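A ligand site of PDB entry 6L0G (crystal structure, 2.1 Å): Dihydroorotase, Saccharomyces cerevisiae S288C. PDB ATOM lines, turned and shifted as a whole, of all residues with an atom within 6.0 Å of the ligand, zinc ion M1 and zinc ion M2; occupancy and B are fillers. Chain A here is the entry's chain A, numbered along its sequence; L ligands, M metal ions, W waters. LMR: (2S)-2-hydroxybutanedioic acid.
Residues that only touch the ligand: Lys 230 (3.5 Å) and Ala 260 (3.5 Å).
Hydrophobic or aromatic side chains that line the ligand: His 16, His 137, Ala 260 and His 262.
Within 4 Å of the ligand: His 16, Arg 18, Asn 43, KCX 98, Thr 105, Thr 106, His 137, His 180, Lys 230, Asp 258, Ala 260, His 262 and Ala 275.
The nearest printed residue that does not touch the ligand is His 14 (4.1 Å).
The side-chain amide nitrogen (ND2) of Asn 43 lies within hydrogen-bond range of an oxygen (O4B) of the ligand.
An oxygen (O4A) of the ligand sits at hydrogen-bond distance from the side-chain hydroxyl (OG1) of Thr 106.
NE2 of His 262 is in hydrogen-bond range of O4A of the ligand, at 3.3 Å.
An oxygen (O4B) of the ligand lies within salt-bridge range of the guanidinium group (NH1) of Arg 18.
An oxygen (O1B) of the ligand is in hydrogen-bond range of the side-chain hydroxyl (OG1) of Thr 105.
An oxygen (O2) of the ligand sits at hydrogen-bond distance from the backbone carbonyl oxygen (O) of Ala 275.
ND2 of Asn 43 lies within hydrogen-bond range of O of Thr 106 (3.0 Å).
OG1 of Thr 106 sits at hydrogen-bond distance from O of Ala 275.
O of Val 277 lies within hydrogen-bond range of N of Ala 260 (2.9 Å).
The guanidinium group of Arg 18 is in hydrogen-bond range of the backbone carbonyl oxygen of Pro 261 (2.8 Å).
The backbone carbonyl oxygen (O) of Asn 43 sits at hydrogen-bond distance from the side-chain amide nitrogen (ND2) of Asn 107 (2.9 Å).
The side-chain amino group (NZ) of Lys 230 sits at hydrogen-bond distance from the backbone carbonyl oxygen (O) of Val 104 (2.8 Å).
N of His 16 sits at hydrogen-bond distance from O of Ser 259.
A ring nitrogen (ND1) of His 16 is in hydrogen-bond range of the side-chain amide oxygen of Asn 43.
Within 4 Å of zinc ion M1: His 14, His 16, KCX 98 and Asp 258.
Along chain A the residues within 4 Å of zinc ion M1 span positions 14 to 258.
Water W1 lies within hydrogen-bond range of O2 of the ligand, O of Lys 230 and OD2 of Asp 258.
Zinc ion M1 is bound by a ring nitrogen (NE2) of His 16 (2.1 Å), a ring nitrogen (NE2) of His 14 (2.1 Å), the side-chain carboxylate of Asp 258 (2.1 Å), OQ1 of KCX 98 (2.2 Å) and an oxygen (O1A) of the ligand (2.3 Å).
Three residues have an atom within 4 Å of zinc ion M2: KCX 98, His 137 and His 180.
OQ2 of KCX 98 binds zinc ion M2 (1.9 Å).
Zinc ion M2 is bound by NE2 of His 180 (2.1 Å).
A ring nitrogen (ND1) of His 137 binds zinc ion M2, 2.2 Å away.
Zinc ion M2 is bound by O1A of the ligand, at 2.5 Å.
Slightly farther from zinc ion M2 lies an oxygen (O1B) of the ligand (2.8 Å).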
ATOM      1  N   HIS A  14     -10.667  35.236  17.143  1.00  0.00           N
ATOM      2  CA  HIS A  14     -10.505  33.765  17.184  1.00  0.00           C
ATOM      3  C   HIS A  14      -9.655  33.339  15.986  1.00  0.00           C
ATOM      4  O   HIS A  14     -10.190  33.087  14.904  1.00  0.00           O
ATOM      5  CB  HIS A  14     -11.874  33.087  17.188  1.00  0.00           C
ATOM      6  CG  HIS A  14     -11.841  31.644  17.649  1.00  0.00           C
ATOM      7  ND1 HIS A  14     -12.736  31.136  18.561  1.00  0.00           N
ATOM      8  CD2 HIS A  14     -11.053  30.608  17.274  1.00  0.00           C
ATOM      9  CE1 HIS A  14     -12.480  29.851  18.750  1.00  0.00           C
ATOM     10  NE2 HIS A  14     -11.479  29.505  17.980  1.00  0.00           N
ATOM     11  N   HIS A  16      -6.307  30.969  14.379  1.00  0.00           N
ATOM     12  CA  HIS A  16      -5.293  29.908  14.405  1.00  0.00           C
ATOM     13  C   HIS A  16      -4.221  30.178  13.354  1.00  0.00           C
ATOM     14  O   HIS A  16      -4.541  30.306  12.164  1.00  0.00           O
ATOM     15  CB  HIS A  16      -5.929  28.537  14.155  1.00  0.00           C
ATOM     16  CG  HIS A  16      -6.928  28.124  15.209  1.00  0.00           C
ATOM     17  ND1 HIS A  16      -6.569  27.409  16.327  1.00  0.00           N
ATOM     18  CD2 HIS A  16      -8.253  28.349  15.305  1.00  0.00           C
ATOM     19  CE1 HIS A  16      -7.642  27.201  17.080  1.00  0.00           C
ATOM     20  NE2 HIS A  16      -8.677  27.767  16.480  1.00  0.00           N
ATOM     21  N   ARG A  18      -0.969  28.283  13.672  1.00  0.00           N
ATOM     22  CA  ARG A  18      -0.124  27.079  13.695  1.00  0.00           C
ATOM     23  C   ARG A  18       1.335  27.452  14.015  1.00  0.00           C
ATOM     24  O   ARG A  18       1.586  28.371  14.814  1.00  0.00           O
ATOM     25  CB  ARG A  18      -0.288  26.307  12.389  1.00  0.00           C
ATOM     26  CG  ARG A  18      -1.755  26.202  11.857  1.00  0.00           C
ATOM     27  CD  ARG A  18      -2.722  25.492  12.837  1.00  0.00           C
ATOM     28  NE  ARG A  18      -3.952  25.104  12.160  1.00  0.00           N
ATOM     29  CZ  ARG A  18      -5.095  24.765  12.748  1.00  0.00           C
ATOM     30  NH1 ARG A  18      -5.197  24.759  14.079  1.00  0.00           N
ATOM     31  NH2 ARG A  18      -6.152  24.436  11.997  1.00  0.00           N
ATOM     32  N   MET A  41      -5.203  31.637  19.227  1.00  0.00           N
ATOM     33  CA  MET A  41      -5.542  30.447  20.007  1.00  0.00           C
ATOM     34  C   MET A  41      -4.308  29.582  20.280  1.00  0.00           C
ATOM     35  O   MET A  41      -3.322  29.663  19.557  1.00  0.00           O
ATOM     36  CB  MET A  41      -6.612  29.654  19.262  1.00  0.00           C
ATOM     37  CG  MET A  41      -7.975  30.400  19.235  1.00  0.00           C
ATOM     38  SD  MET A  41      -8.535  30.661  20.921  1.00  0.00           S
ATOM     39  CE  MET A  41     -10.036  31.604  20.779  1.00  0.00           C
ATOM     40  N   ASN A  43      -3.888  26.001  20.689  1.00  0.00           N
ATOM     41  CA  ASN A  43      -3.947  24.544  20.537  1.00  0.00           C
ATOM     42  C   ASN A  43      -2.849  24.056  19.567  1.00  0.00           C
ATOM     43  O   ASN A  43      -3.104  23.433  18.541  1.00  0.00           O
ATOM     44  CB  ASN A  43      -5.340  24.102  20.096  1.00  0.00           C
ATOM     45  CG  ASN A  43      -5.736  24.642  18.727  1.00  0.00           C
ATOM     46  OD1 ASN A  43      -5.240  25.677  18.296  1.00  0.00           O
ATOM     47  ND2 ASN A  43      -6.622  23.928  18.032  1.00  0.00           N
ATOM     48  N   KCX A  98      -8.082  29.554  26.906  1.00  0.00           N
ATOM     49  CA  KCX A  98      -9.025  28.892  26.014  1.00  0.00           C
ATOM     50  CB  KCX A  98      -8.511  28.867  24.570  1.00  0.00           C
ATOM     51  CG  KCX A  98      -9.339  27.978  23.644  1.00  0.00           C
ATOM     52  CD  KCX A  98     -10.727  28.584  23.429  1.00  0.00           C
ATOM     53  CE  KCX A  98     -11.493  27.867  22.325  1.00  0.00           C
ATOM     54  NZ  KCX A  98     -10.605  27.803  21.147  1.00  0.00           N
ATOM     55  C   KCX A  98      -9.293  27.468  26.460  1.00  0.00           C
ATOM     56  O   KCX A  98      -8.360  26.689  26.644  1.00  0.00           O
ATOM     57  CX  KCX A  98     -11.018  27.266  20.005  1.00  0.00           C
ATOM     58  OQ1 KCX A  98     -10.232  27.210  19.050  1.00  0.00           O
ATOM     59  OQ2 KCX A  98     -12.156  26.783  19.902  1.00  0.00           O
ATOM     60  N   TYR A 100     -10.686  23.789  25.596  1.00  0.00           N
ATOM     61  CA  TYR A 100     -11.081  22.756  24.652  1.00  0.00           C
ATOM     62  C   TYR A 100     -11.595  21.541  25.417  1.00  0.00           C
ATOM     63  O   TYR A 100     -10.852  20.996  26.231  1.00  0.00           O
ATOM     64  CB  TYR A 100      -9.895  22.330  23.749  1.00  0.00           C
ATOM     65  CG  TYR A 100      -9.374  23.429  22.838  1.00  0.00           C
ATOM     66  CD1 TYR A 100      -9.988  23.693  21.639  1.00  0.00           C
ATOM     67  CD2 TYR A 100      -8.272  24.202  23.219  1.00  0.00           C
ATOM     68  CE1 TYR A 100      -9.506  24.698  20.816  1.00  0.00           C
ATOM     69  CE2 TYR A 100      -7.797  25.201  22.406  1.00  0.00           C
ATOM     70  CZ  TYR A 100      -8.410  25.453  21.199  1.00  0.00           C
ATOM     71  OH  TYR A 100      -7.935  26.463  20.393  1.00  0.00           O
ATOM     72  N   VAL A 104     -12.965  16.922  21.122  1.00  0.00           N
ATOM     73  CA  VAL A 104     -14.024  17.445  20.253  1.00  0.00           C
ATOM     74  C   VAL A 104     -13.481  18.147  19.008  1.00  0.00           C
ATOM     75  O   VAL A 104     -14.256  18.335  18.051  1.00  0.00           O
ATOM     76  CB  VAL A 104     -14.992  18.393  20.988  1.00  0.00           C
ATOM     77  CG1 VAL A 104     -15.667  17.677  22.166  1.00  0.00           C
ATOM     78  CG2 VAL A 104     -14.285  19.658  21.466  1.00  0.00           C
ATOM     79  N   THR A 105     -12.199  18.498  18.963  1.00  0.00           N
ATOM     80  CA  THR A 105     -11.701  19.225  17.794  1.00  0.00           C
ATOM     81  C   THR A 105     -10.179  19.112  17.699  1.00  0.00           C
ATOM     82  O   THR A 105      -9.543  18.304  18.390  1.00  0.00           O
ATOM     83  CB  THR A 105     -12.161  20.685  17.849  1.00  0.00           C
ATOM     84  OG1 THR A 105     -11.928  21.303  16.592  1.00  0.00           O
ATOM     85  CG2 THR A 105     -11.444  21.450  18.941  1.00  0.00           C
ATOM     86  N   THR A 106      -9.597  19.902  16.786  1.00  0.00           N
ATOM     87  CA  THR A 106      -8.174  19.832  16.478  1.00  0.00           C
ATOM     88  C   THR A 106      -7.316  20.085  17.724  1.00  0.00           C
ATOM     89  O   THR A 106      -7.475  21.104  18.404  1.00  0.00           O
ATOM     90  CB  THR A 106      -7.810  20.874  15.411  1.00  0.00           C
ATOM     91  OG1 THR A 106      -8.591  20.653  14.213  1.00  0.00           O
ATOM     92  CG2 THR A 106      -6.347  20.797  15.067  1.00  0.00           C
ATOM     93  N   ASN A 107      -6.388  19.157  17.991  1.00  0.00           N
ATOM     94  CA  ASN A 107      -5.427  19.272  19.096  1.00  0.00           C
ATOM     95  C   ASN A 107      -6.123  19.520  20.433  1.00  0.00           C
ATOM     96  O   ASN A 107      -5.705  20.360  21.247  1.00  0.00           O
ATOM     97  CB  ASN A 107      -4.393  20.355  18.800  1.00  0.00           C
ATOM     98  CG  ASN A 107      -3.438  19.944  17.678  1.00  0.00           C
ATOM     99  OD1 ASN A 107      -3.304  18.764  17.380  1.00  0.00           O
ATOM    100  ND2 ASN A 107      -2.782  20.931  17.049  1.00  0.00           N
ATOM    101  N   HIS A 137     -14.691  26.608  23.917  1.00  0.00           N
ATOM    102  CA  HIS A 137     -15.233  25.842  22.803  1.00  0.00           C
ATOM    103  C   HIS A 137     -16.372  25.045  23.415  1.00  0.00           C
ATOM    104  O   HIS A 137     -16.179  23.988  24.011  1.00  0.00           O
ATOM    105  CB  HIS A 137     -14.181  24.949  22.158  1.00  0.00           C
ATOM    106  CG  HIS A 137     -14.713  24.142  21.002  1.00  0.00           C
ATOM    107  ND1 HIS A 137     -14.106  24.139  19.751  1.00  0.00           N
ATOM    108  CD2 HIS A 137     -15.788  23.328  20.903  1.00  0.00           C
ATOM    109  CE1 HIS A 137     -14.785  23.339  18.946  1.00  0.00           C
ATOM    110  NE2 HIS A 137     -15.804  22.826  19.624  1.00  0.00           N
ATOM    111  N   GLU A 179     -17.304  30.734  22.210  1.00  0.00           N
ATOM    112  CA  GLU A 179     -16.698  30.905  20.901  1.00  0.00           C
ATOM    113  C   GLU A 179     -17.559  30.255  19.816  1.00  0.00           C
ATOM    114  O   GLU A 179     -18.319  29.316  20.070  1.00  0.00           O
ATOM    115  CB  GLU A 179     -15.298  30.276  20.857  1.00  0.00           C
ATOM    116  CG  GLU A 179     -14.275  30.925  21.788  1.00  0.00           C
ATOM    117  CD  GLU A 179     -13.943  32.354  21.403  1.00  0.00           C
ATOM    118  OE1 GLU A 179     -14.079  32.694  20.204  1.00  0.00           O
ATOM    119  OE2 GLU A 179     -13.542  33.135  22.305  1.00  0.00           O
ATOM    120  N   HIS A 180     -17.428  30.786  18.593  1.00  0.00           N
ATOM    121  CA  HIS A 180     -18.060  30.286  17.378  1.00  0.00           C
ATOM    122  C   HIS A 180     -19.403  29.617  17.628  1.00  0.00           C
ATOM    123  O   HIS A 180     -19.524  28.389  17.523  1.00  0.00           O
ATOM    124  CB  HIS A 180     -17.112  29.350  16.597  1.00  0.00           C
ATOM    125  CG  HIS A 180     -16.338  28.371  17.441  1.00  0.00           C
ATOM    126  ND1 HIS A 180     -16.913  27.667  18.479  1.00  0.00           N
ATOM    127  CD2 HIS A 180     -15.073  27.923  17.356  1.00  0.00           C
ATOM    128  CE1 HIS A 180     -16.021  26.857  19.015  1.00  0.00           C
ATOM    129  NE2 HIS A 180     -14.890  27.001  18.361  1.00  0.00           N
ATOM    130  N   CYS A 229     -16.086  21.663   9.933  1.00  0.00           N
ATOM    131  CA  CYS A 229     -15.409  22.315  11.037  1.00  0.00           C
ATOM    132  C   CYS A 229     -16.140  21.939  12.313  1.00  0.00           C
ATOM    133  O   CYS A 229     -17.237  21.373  12.261  1.00  0.00           O
ATOM    134  CB  CYS A 229     -15.370  23.845  10.822  1.00  0.00           C
ATOM    135  SG  CYS A 229     -17.016  24.611  10.923  1.00  0.00           S
ATOM    136  N   LYS A 230     -15.544  22.296  13.472  1.00  0.00           N
ATOM    137  CA  LYS A 230     -16.248  22.198  14.741  1.00  0.00           C
ATOM    138  C   LYS A 230     -16.465  23.591  15.340  1.00  0.00           C
ATOM    139  O   LYS A 230     -15.576  24.438  15.234  1.00  0.00           O
ATOM    140  CB  LYS A 230     -15.469  21.329  15.726  1.00  0.00           C
ATOM    141  CG  LYS A 230     -15.312  19.862  15.313  1.00  0.00           C
ATOM    142  CD  LYS A 230     -16.668  19.232  15.029  1.00  0.00           C
ATOM    143  CE  LYS A 230     -17.326  18.834  16.331  1.00  0.00           C
ATOM    144  NZ  LYS A 230     -16.685  17.582  16.897  1.00  0.00           N
ATOM    145  N   PRO A 231     -17.634  23.872  15.951  1.00  0.00           N
ATOM    146  CA  PRO A 231     -18.860  23.048  15.867  1.00  0.00           C
ATOM    147  C   PRO A 231     -19.385  22.997  14.432  1.00  0.00           C
ATOM    148  O   PRO A 231     -19.145  23.946  13.662  1.00  0.00           O
ATOM    149  CB  PRO A 231     -19.850  23.772  16.810  1.00  0.00           C
ATOM    150  CG  PRO A 231     -19.018  24.860  17.527  1.00  0.00           C
ATOM    151  CD  PRO A 231     -17.931  25.185  16.547  1.00  0.00           C
ATOM    152  N   ASP A 258     -12.410  31.974  13.680  1.00  0.00           N
ATOM    153  CA  ASP A 258     -11.941  30.607  13.817  1.00  0.00           C
ATOM    154  C   ASP A 258     -11.314  30.111  12.516  1.00  0.00           C
ATOM    155  O   ASP A 258     -11.495  28.965  12.103  1.00  0.00           O
ATOM    156  CB  ASP A 258     -13.070  29.660  14.260  1.00  0.00           C
ATOM    157  CG  ASP A 258     -12.555  28.265  14.673  1.00  0.00           C
ATOM    158  OD1 ASP A 258     -11.360  28.133  14.990  1.00  0.00           O
ATOM    159  OD2 ASP A 258     -13.365  27.302  14.653  1.00  0.00           O
ATOM    160  N   SER A 259     -10.575  31.000  11.849  1.00  0.00           N
ATOM    161  CA  SER A 259      -9.816  30.557  10.683  1.00  0.00           C
ATOM    162  C   SER A 259      -8.798  29.511  11.134  1.00  0.00           C
ATOM    163  O   SER A 259      -8.011  29.762  12.046  1.00  0.00           O
ATOM    164  CB  SER A 259      -9.128  31.731  10.007  1.00  0.00           C
ATOM    165  OG  SER A 259      -8.290  31.283   8.955  1.00  0.00           O
ATOM    166  N   ALA A 260      -8.877  28.329  10.528  1.00  0.00           N
ATOM    167  CA  ALA A 260      -8.154  27.133  10.991  1.00  0.00           C
ATOM    168  C   ALA A 260      -7.444  26.472   9.817  1.00  0.00           C
ATOM    169  O   ALA A 260      -8.017  25.596   9.146  1.00  0.00           O
ATOM    170  CB  ALA A 260      -9.108  26.160  11.664  1.00  0.00           C
ATOM    171  N   PRO A 261      -6.194  26.851   9.536  1.00  0.00           N
ATOM    172  CA  PRO A 261      -5.516  26.327   8.344  1.00  0.00           C
ATOM    173  C   PRO A 261      -5.129  24.862   8.494  1.00  0.00           C
ATOM    174  O   PRO A 261      -4.600  24.438   9.519  1.00  0.00           O
ATOM    175  CB  PRO A 261      -4.275  27.205   8.206  1.00  0.00           C
ATOM    176  CG  PRO A 261      -4.086  27.861   9.510  1.00  0.00           C
ATOM    177  CD  PRO A 261      -5.353  27.801  10.294  1.00  0.00           C
ATOM    178  N   HIS A 262      -5.385  24.086   7.430  1.00  0.00           N
ATOM    179  CA  HIS A 262      -4.938  22.706   7.290  1.00  0.00           C
ATOM    180  C   HIS A 262      -4.383  22.501   5.890  1.00  0.00           C
ATOM    181  O   HIS A 262      -4.973  22.994   4.910  1.00  0.00           O
ATOM    182  CB  HIS A 262      -6.089  21.722   7.530  1.00  0.00           C
ATOM    183  CG  HIS A 262      -6.594  21.719   8.941  1.00  0.00           C
ATOM    184  ND1 HIS A 262      -5.880  21.134   9.967  1.00  0.00           N
ATOM    185  CD2 HIS A 262      -7.713  22.220   9.492  1.00  0.00           C
ATOM    186  CE1 HIS A 262      -6.547  21.285  11.106  1.00  0.00           C
ATOM    187  NE2 HIS A 262      -7.662  21.938  10.842  1.00  0.00           N
ATOM    188  N   ALA A 275     -10.877  19.038  11.158  1.00  0.00           N
ATOM    189  CA  ALA A 275     -11.925  20.030  11.270  1.00  0.00           C
ATOM    190  C   ALA A 275     -11.340  21.429  11.141  1.00  0.00           C
ATOM    191  O   ALA A 275     -10.331  21.753  11.782  1.00  0.00           O
ATOM    192  CB  ALA A 275     -12.644  19.892  12.612  1.00  0.00           C
ATOM    193  N   GLY A 276     -11.990  22.265  10.357  1.00  0.00           N
ATOM    194  CA  GLY A 276     -11.565  23.651  10.262  1.00  0.00           C
ATOM    195  C   GLY A 276     -11.718  24.276   8.899  1.00  0.00           C
ATOM    196  O   GLY A 276     -11.471  23.635   7.863  1.00  0.00           O
ATOM    197  N   VAL A 277     -12.133  25.543   8.891  1.00  0.00           N
ATOM    198  CA  VAL A 277     -12.329  26.317   7.672  1.00  0.00           C
ATOM    199  C   VAL A 277     -11.305  27.440   7.687  1.00  0.00           C
ATOM    200  O   VAL A 277     -11.162  28.124   8.715  1.00  0.00           O
ATOM    201  CB  VAL A 277     -13.769  26.872   7.594  1.00  0.00           C
ATOM    202  CG1 VAL A 277     -13.939  27.799   6.390  1.00  0.00           C
ATOM    203  CG2 VAL A 277     -14.784  25.731   7.531  1.00  0.00           C
HETATM  204  C1  LMR L   1     -11.585  24.441  16.348  1.00  0.00           C
HETATM  205  O1A LMR L   1     -11.672  25.674  16.608  1.00  0.00           O
HETATM  206  O1B LMR L   1     -12.495  23.713  16.784  1.00  0.00           O
HETATM  207  C2  LMR L   1     -10.427  23.831  15.527  1.00  0.00           C
HETATM  208  O2  LMR L   1     -10.772  23.309  14.265  1.00  0.00           O
HETATM  209  C3  LMR L   1      -9.499  24.935  15.179  1.00  0.00           C
HETATM  210  C4  LMR L   1      -8.283  24.184  14.704  1.00  0.00           C
HETATM  211  O4A LMR L   1      -8.322  23.392  13.706  1.00  0.00           O
HETATM  212  O4B LMR L   1      -7.247  24.436  15.365  1.00  0.00           O
HETATM  213 ZN    ZN M   1     -10.738  27.756  17.001  1.00  0.00          ZN
HETATM  214 ZN    ZN M   2     -13.191  25.748  18.641  1.00  0.00          ZN
HETATM  215  O   HOH W   1     -13.233  24.364  13.431  1.00  0.00           O
